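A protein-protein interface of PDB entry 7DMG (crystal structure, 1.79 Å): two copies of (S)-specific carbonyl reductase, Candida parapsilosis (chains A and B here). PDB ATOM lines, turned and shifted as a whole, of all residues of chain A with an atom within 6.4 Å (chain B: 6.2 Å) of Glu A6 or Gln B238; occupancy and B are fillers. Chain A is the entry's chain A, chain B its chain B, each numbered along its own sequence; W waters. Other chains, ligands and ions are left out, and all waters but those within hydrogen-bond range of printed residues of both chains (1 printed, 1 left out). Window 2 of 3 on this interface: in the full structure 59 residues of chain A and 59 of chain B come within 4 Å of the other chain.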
ATOM      1  N   SER A   1      29.502  25.752  20.434  1.00  0.00           N
ATOM      2  CA  SER A   1      28.681  25.142  19.398  1.00  0.00           C
ATOM      3  C   SER A   1      28.687  23.612  19.499  1.00  0.00           C
ATOM      4  O   SER A   1      28.046  22.938  18.691  1.00  0.00           O
ATOM      5  CB  SER A   1      29.157  25.578  18.010  1.00  0.00           C
ATOM      6  OG  SER A   1      28.384  24.978  16.977  1.00  0.00           O
ATOM      7  N   GLU A   4      25.553  20.975  18.736  1.00  0.00           N
ATOM      8  CA  GLU A   4      24.631  21.649  17.840  1.00  0.00           C
ATOM      9  C   GLU A   4      25.213  21.572  16.438  1.00  0.00           C
ATOM     10  O   GLU A   4      26.414  21.813  16.240  1.00  0.00           O
ATOM     11  CB  GLU A   4      24.391  23.095  18.323  1.00  0.00           C
ATOM     12  CG  GLU A   4      23.615  22.967  19.671  1.00  0.00           C
ATOM     13  CD  GLU A   4      23.194  24.190  20.477  1.00  0.00           C
ATOM     14  OE1 GLU A   4      23.085  25.371  20.838  1.00  0.00           O
ATOM     15  OE2 GLU A   4      23.976  24.724  19.654  1.00  0.00           O
ATOM     16  N   ILE A   5      24.382  21.126  15.499  1.00  0.00           N
ATOM     17  CA  ILE A   5      24.664  21.091  14.071  1.00  0.00           C
ATOM     18  C   ILE A   5      24.456  22.515  13.593  1.00  0.00           C
ATOM     19  O   ILE A   5      23.332  23.030  13.656  1.00  0.00           O
ATOM     20  CB  ILE A   5      23.693  20.144  13.355  1.00  0.00           C
ATOM     21  CG1 ILE A   5      23.833  18.711  13.864  1.00  0.00           C
ATOM     22  CG2 ILE A   5      23.874  20.215  11.847  1.00  0.00           C
ATOM     23  CD1 ILE A   5      22.593  17.856  13.553  1.00  0.00           C
ATOM     24  N   GLU A   6      25.505  23.180  13.126  1.00  0.00           N
ATOM     25  CA  GLU A   6      25.173  24.516  12.689  1.00  0.00           C
ATOM     26  C   GLU A   6      25.397  24.585  11.185  1.00  0.00           C
ATOM     27  O   GLU A   6      26.137  23.788  10.593  1.00  0.00           O
ATOM     28  CB  GLU A   6      25.955  25.594  13.448  1.00  0.00           C
ATOM     29  CG  GLU A   6      27.387  25.860  13.154  1.00  0.00           C
ATOM     30  CD  GLU A   6      27.765  27.251  13.712  1.00  0.00           C
ATOM     31  OE1 GLU A   6      28.793  27.820  13.290  1.00  0.00           O
ATOM     32  OE2 GLU A   6      27.137  27.676  14.723  1.00  0.00           O
ATOM     33  N   SER A   7      24.697  25.520  10.577  1.00  0.00           N
ATOM     34  CA  SER A   7      24.555  25.551   9.130  1.00  0.00           C
ATOM     35  C   SER A   7      25.876  25.923   8.472  1.00  0.00           C
ATOM     36  O   SER A   7      26.672  26.686   9.023  1.00  0.00           O
ATOM     37  CB  SER A   7      23.480  26.564   8.756  1.00  0.00           C
ATOM     38  OG  SER A   7      23.389  26.783   7.339  1.00  0.00           O
ATOM     39  N   TYR A   8      26.108  25.369   7.279  1.00  0.00           N
ATOM     40  CA  TYR A   8      27.176  25.844   6.413  1.00  0.00           C
ATOM     41  C   TYR A   8      26.735  27.052   5.594  1.00  0.00           C
ATOM     42  O   TYR A   8      27.581  27.737   5.010  1.00  0.00           O
ATOM     43  CB  TYR A   8      27.630  24.719   5.461  1.00  0.00           C
ATOM     44  CG  TYR A   8      28.721  23.819   6.019  1.00  0.00           C
ATOM     45  CD1 TYR A   8      28.726  23.451   7.360  1.00  0.00           C
ATOM     46  CD2 TYR A   8      29.746  23.332   5.205  1.00  0.00           C
ATOM     47  CE1 TYR A   8      29.716  22.642   7.879  1.00  0.00           C
ATOM     48  CE2 TYR A   8      30.743  22.501   5.725  1.00  0.00           C
ATOM     49  CZ  TYR A   8      30.719  22.169   7.061  1.00  0.00           C
ATOM     50  OH  TYR A   8      31.693  21.361   7.608  1.00  0.00           O
ATOM     51  N   CYS A   9      25.431  27.326   5.538  1.00  0.00           N
ATOM     52  CA  CYS A   9      24.923  28.449   4.748  1.00  0.00           C
ATOM     53  C   CYS A   9      24.806  29.723   5.571  1.00  0.00           C
ATOM     54  O   CYS A   9      25.186  30.802   5.107  1.00  0.00           O
ATOM     55  CB  CYS A   9      23.558  28.128   4.127  1.00  0.00           C
ATOM     56  SG  CYS A   9      23.459  26.677   3.067  1.00  0.00           S
ATOM     57  N   ASN A  10      24.281  29.614   6.793  1.00  0.00           N
ATOM     58  CA  ASN A  10      23.932  30.798   7.574  1.00  0.00           C
ATOM     59  C   ASN A  10      23.706  30.348   9.016  1.00  0.00           C
ATOM     60  O   ASN A  10      22.639  29.823   9.339  1.00  0.00           O
ATOM     61  CB  ASN A  10      22.700  31.475   6.996  1.00  0.00           C
ATOM     62  CG  ASN A  10      22.459  32.844   7.589  1.00  0.00           C
ATOM     63  OD1 ASN A  10      22.970  33.165   8.660  1.00  0.00           O
ATOM     64  ND2 ASN A  10      21.667  33.657   6.900  1.00  0.00           N
ATOM     65  N   LYS A  11      24.706  30.566   9.870  1.00  0.00           N
ATOM     66  CA  LYS A  11      24.607  30.118  11.258  1.00  0.00           C
ATOM     67  C   LYS A  11      23.524  30.850  12.050  1.00  0.00           C
ATOM     68  O   LYS A  11      23.173  30.404  13.145  1.00  0.00           O
ATOM     69  CB  LYS A  11      25.965  30.256  11.937  1.00  0.00           C
ATOM     70  CG  LYS A  11      26.473  31.678  12.014  1.00  0.00           C
ATOM     71  CD  LYS A  11      27.663  31.786  12.970  1.00  0.00           C
ATOM     72  CE  LYS A  11      28.336  33.147  12.846  1.00  0.00           C
ATOM     73  NZ  LYS A  11      29.779  33.091  13.220  1.00  0.00           N
ATOM     74  N   GLY A  14      20.480  28.975  13.605  1.00  0.00           N
ATOM     75  CA  GLY A  14      20.524  28.334  14.898  1.00  0.00           C
ATOM     76  C   GLY A  14      20.645  26.831  14.752  1.00  0.00           C
ATOM     77  O   GLY A  14      20.867  26.304  13.651  1.00  0.00           O
ATOM     78  N   PRO A  15      20.480  26.112  15.864  1.00  0.00           N
ATOM     79  CA  PRO A  15      20.652  24.650  15.849  1.00  0.00           C
ATOM     80  C   PRO A  15      19.738  23.978  14.834  1.00  0.00           C
ATOM     81  O   PRO A  15      18.529  24.219  14.802  1.00  0.00           O
ATOM     82  CB  PRO A  15      20.293  24.238  17.281  1.00  0.00           C
ATOM     83  CG  PRO A  15      20.517  25.468  18.105  1.00  0.00           C
ATOM     84  CD  PRO A  15      20.184  26.632  17.209  1.00  0.00           C
ATOM     85  N   LEU A  16      20.331  23.117  14.001  1.00  0.00           N
ATOM     86  CA  LEU A  16      19.575  22.468  12.939  1.00  0.00           C
ATOM     87  C   LEU A  16      19.008  21.126  13.412  1.00  0.00           C
ATOM     88  O   LEU A  16      19.570  20.491  14.312  1.00  0.00           O
ATOM     89  CB  LEU A  16      20.470  22.254  11.720  1.00  0.00           C
ATOM     90  CG  LEU A  16      21.031  23.525  11.085  1.00  0.00           C
ATOM     91  CD1 LEU A  16      21.783  23.182   9.805  1.00  0.00           C
ATOM     92  CD2 LEU A  16      19.898  24.536  10.791  1.00  0.00           C
ATOM     93  N   LYS B 233      21.855  13.023   6.969  1.00  0.00           N
ATOM     94  CA  LYS B 233      20.900  14.118   6.884  1.00  0.00           C
ATOM     95  C   LYS B 233      21.403  15.376   7.550  1.00  0.00           C
ATOM     96  O   LYS B 233      20.973  16.468   7.176  1.00  0.00           O
ATOM     97  CB  LYS B 233      19.571  13.786   7.516  1.00  0.00           C
ATOM     98  CG  LYS B 233      18.870  12.631   6.958  1.00  0.00           C
ATOM     99  CD  LYS B 233      17.434  12.990   7.148  1.00  0.00           C
ATOM    100  CE  LYS B 233      16.629  11.851   7.626  1.00  0.00           C
ATOM    101  NZ  LYS B 233      15.238  12.292   7.837  1.00  0.00           N
ATOM    102  N   ALA B 234      22.232  15.248   8.587  1.00  0.00           N
ATOM    103  CA  ALA B 234      22.789  16.449   9.194  1.00  0.00           C
ATOM    104  C   ALA B 234      23.497  17.293   8.141  1.00  0.00           C
ATOM    105  O   ALA B 234      23.362  18.521   8.123  1.00  0.00           O
ATOM    106  CB  ALA B 234      23.738  16.081  10.338  1.00  0.00           C
ATOM    107  N   LYS B 235      24.228  16.640   7.233  1.00  0.00           N
ATOM    108  CA  LYS B 235      24.912  17.369   6.169  1.00  0.00           C
ATOM    109  C   LYS B 235      23.921  17.959   5.175  1.00  0.00           C
ATOM    110  O   LYS B 235      24.134  19.071   4.673  1.00  0.00           O
ATOM    111  CB  LYS B 235      25.924  16.458   5.471  1.00  0.00           C
ATOM    112  CG  LYS B 235      27.073  16.022   6.397  1.00  0.00           C
ATOM    113  CD  LYS B 235      28.167  15.344   5.601  1.00  0.00           C
ATOM    114  CE  LYS B 235      29.297  14.896   6.480  1.00  0.00           C
ATOM    115  NZ  LYS B 235      29.014  13.589   7.118  1.00  0.00           N
ATOM    116  N   TRP B 236      22.827  17.244   4.883  1.00  0.00           N
ATOM    117  CA  TRP B 236      21.770  17.838   4.065  1.00  0.00           C
ATOM    118  C   TRP B 236      21.259  19.124   4.696  1.00  0.00           C
ATOM    119  O   TRP B 236      21.138  20.149   4.025  1.00  0.00           O
ATOM    120  CB  TRP B 236      20.593  16.886   3.890  1.00  0.00           C
ATOM    121  CG  TRP B 236      20.868  15.602   3.215  1.00  0.00           C
ATOM    122  CD1 TRP B 236      22.015  15.220   2.594  1.00  0.00           C
ATOM    123  CD2 TRP B 236      19.940  14.528   3.058  1.00  0.00           C
ATOM    124  NE1 TRP B 236      21.870  13.947   2.085  1.00  0.00           N
ATOM    125  CE2 TRP B 236      20.598  13.510   2.353  1.00  0.00           C
ATOM    126  CE3 TRP B 236      18.610  14.330   3.452  1.00  0.00           C
ATOM    127  CZ2 TRP B 236      19.968  12.325   2.009  1.00  0.00           C
ATOM    128  CZ3 TRP B 236      17.989  13.139   3.122  1.00  0.00           C
ATOM    129  CH2 TRP B 236      18.673  12.147   2.414  1.00  0.00           C
ATOM    130  N   TRP B 237      20.935  19.079   5.992  1.00  0.00           N
ATOM    131  CA  TRP B 237      20.435  20.271   6.672  1.00  0.00           C
ATOM    132  C   TRP B 237      21.443  21.405   6.586  1.00  0.00           C
ATOM    133  O   TRP B 237      21.073  22.561   6.337  1.00  0.00           O
ATOM    134  CB  TRP B 237      20.126  19.963   8.145  1.00  0.00           C
ATOM    135  CG  TRP B 237      19.143  18.859   8.367  1.00  0.00           C
ATOM    136  CD1 TRP B 237      18.169  18.433   7.508  1.00  0.00           C
ATOM    137  CD2 TRP B 237      19.048  18.020   9.531  1.00  0.00           C
ATOM    138  NE1 TRP B 237      17.473  17.379   8.067  1.00  0.00           N
ATOM    139  CE2 TRP B 237      17.988  17.115   9.309  1.00  0.00           C
ATOM    140  CE3 TRP B 237      19.760  17.944  10.735  1.00  0.00           C
ATOM    141  CZ2 TRP B 237      17.627  16.140  10.247  1.00  0.00           C
ATOM    142  CZ3 TRP B 237      19.392  16.980  11.674  1.00  0.00           C
ATOM    143  CH2 TRP B 237      18.331  16.093  11.420  1.00  0.00           C
ATOM    144  N   GLN B 238      22.728  21.087   6.756  1.00  0.00           N
ATOM    145  CA  GLN B 238      23.750  22.128   6.749  1.00  0.00           C
ATOM    146  C   GLN B 238      23.875  22.811   5.397  1.00  0.00           C
ATOM    147  O   GLN B 238      24.308  23.963   5.336  1.00  0.00           O
ATOM    148  CB  GLN B 238      25.104  21.551   7.125  1.00  0.00           C
ATOM    149  CG  GLN B 238      25.216  21.138   8.584  1.00  0.00           C
ATOM    150  CD  GLN B 238      26.561  20.553   8.871  1.00  0.00           C
ATOM    151  OE1 GLN B 238      26.971  19.595   8.210  1.00  0.00           O
ATOM    152  NE2 GLN B 238      27.259  21.092   9.878  1.00  0.00           N
ATOM    153  N   LEU B 239      23.566  22.107   4.309  1.00  0.00           N
ATOM    154  CA  LEU B 239      23.695  22.647   2.959  1.00  0.00           C
ATOM    155  C   LEU B 239      22.390  23.220   2.418  1.00  0.00           C
ATOM    156  O   LEU B 239      22.373  23.711   1.287  1.00  0.00           O
ATOM    157  CB  LEU B 239      24.210  21.564   2.002  1.00  0.00           C
ATOM    158  CG  LEU B 239      25.592  20.990   2.321  1.00  0.00           C
ATOM    159  CD1 LEU B 239      25.981  19.867   1.342  1.00  0.00           C
ATOM    160  CD2 LEU B 239      26.600  22.114   2.306  1.00  0.00           C
ATOM    161  N   THR B 240      21.303  23.155   3.194  1.00  0.00           N
ATOM    162  CA  THR B 240      19.994  23.649   2.781  1.00  0.00           C
ATOM    163  C   THR B 240      19.767  25.023   3.387  1.00  0.00           C
ATOM    164  O   THR B 240      19.702  25.130   4.623  1.00  0.00           O
ATOM    165  CB  THR B 240      18.886  22.701   3.241  1.00  0.00           C
ATOM    166  OG1 THR B 240      19.119  21.381   2.726  1.00  0.00           O
ATOM    167  CG2 THR B 240      17.516  23.204   2.738  1.00  0.00           C
ATOM    168  N   PRO B 241      19.624  26.082   2.584  1.00  0.00           N
ATOM    169  CA  PRO B 241      19.428  27.428   3.155  1.00  0.00           C
ATOM    170  C   PRO B 241      18.303  27.537   4.168  1.00  0.00           C
ATOM    171  O   PRO B 241      18.464  28.269   5.147  1.00  0.00           O
ATOM    172  CB  PRO B 241      19.155  28.284   1.911  1.00  0.00           C
ATOM    173  CG  PRO B 241      20.006  27.635   0.870  1.00  0.00           C
ATOM    174  CD  PRO B 241      19.881  26.141   1.132  1.00  0.00           C
ATOM    175  N   GLY B 243      17.414  25.215   6.201  1.00  0.00           N
ATOM    176  CA  GLY B 243      17.882  24.529   7.399  1.00  0.00           C
ATOM    177  C   GLY B 243      17.113  23.285   7.789  1.00  0.00           C
ATOM    178  O   GLY B 243      17.267  22.815   8.924  1.00  0.00           O
HETATM  179  O   HOH W   1      27.968  21.598  13.122  1.00  0.00           O
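The backbone carbonyl oxygen of Ile A5 lies within hydrogen-bond range of the backbone NH of Leu A16 (3.0 Å).
The backbone NH of Asn A10 lies within hydrogen-bond range of the side-chain hydroxyl of Ser A7 (3.0 Å).
The backbone NH (N) of Cys A9 is in hydrogen-bond range of the side-chain hydroxyl (OG) of Ser A7 (2.8 Å).
No position is printed for both chains.
Of the 12 pairs that touch across the chains among the printed residues, none has its exchanged pair printed and touching as well.
Hydrophobic or aromatic side chains of chain A that line the printed part of chain B: Ile A5, Tyr A8 and Leu A16.
Along chain A the printed residues that touch a printed residue of chain B span positions 5 to 16.
Among the printed residues, merely in contact across the chains: Ile A5 with Ala B234, Ile A5 with Trp B237, Ile A5 with Gln B238, Ser A7 with Gln B238, Cys A9 with Pro B241, Leu A16 with Trp B237, Leu A16 with Gln B238 and Leu A16 with Gly B243.
Of chain B, only Gln B238 (3.0 Å) comes within 4 Å of Glu A6.
Gln B238 touches six residues of chain A.
Of the printed residues of chain B, Leu A16 touches Trp B237, Gln B238 and Gly B243.
Of the printed residues of chain B, Ser A7 touches Gln B238 (3.6 Å).
Trp B236 touches none of the printed residues of chain A.
The nearest printed residue of chain B that does not touch Glu A6 is Ala B234 (6.4 Å).
The backbone carbonyl oxygen (O) of Glu A6 lies within hydrogen-bond range of the side-chain amide nitrogen (NE2) of Gln B238 (3.0 Å).
The backbone carbonyl oxygen (O) of Leu B239 lies within hydrogen-bond range of the side-chain sulfur (SG) of Cys A9 (3.6 Å).
The backbone NH (N) of Tyr A8 sits at hydrogen-bond distance from the backbone carbonyl oxygen (O) of Gln B238, 3.0 Å away.
O of Gln B238 sits at hydrogen-bond distance from SG of Cys A9, at 3.6 Å.
Water W1 lies within hydrogen-bond range of the backbone NH (N) of Glu A6, the side-chain amide nitrogen (NE2) of Gln B238 and the backbone carbonyl oxygen (O) of Glu A4.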
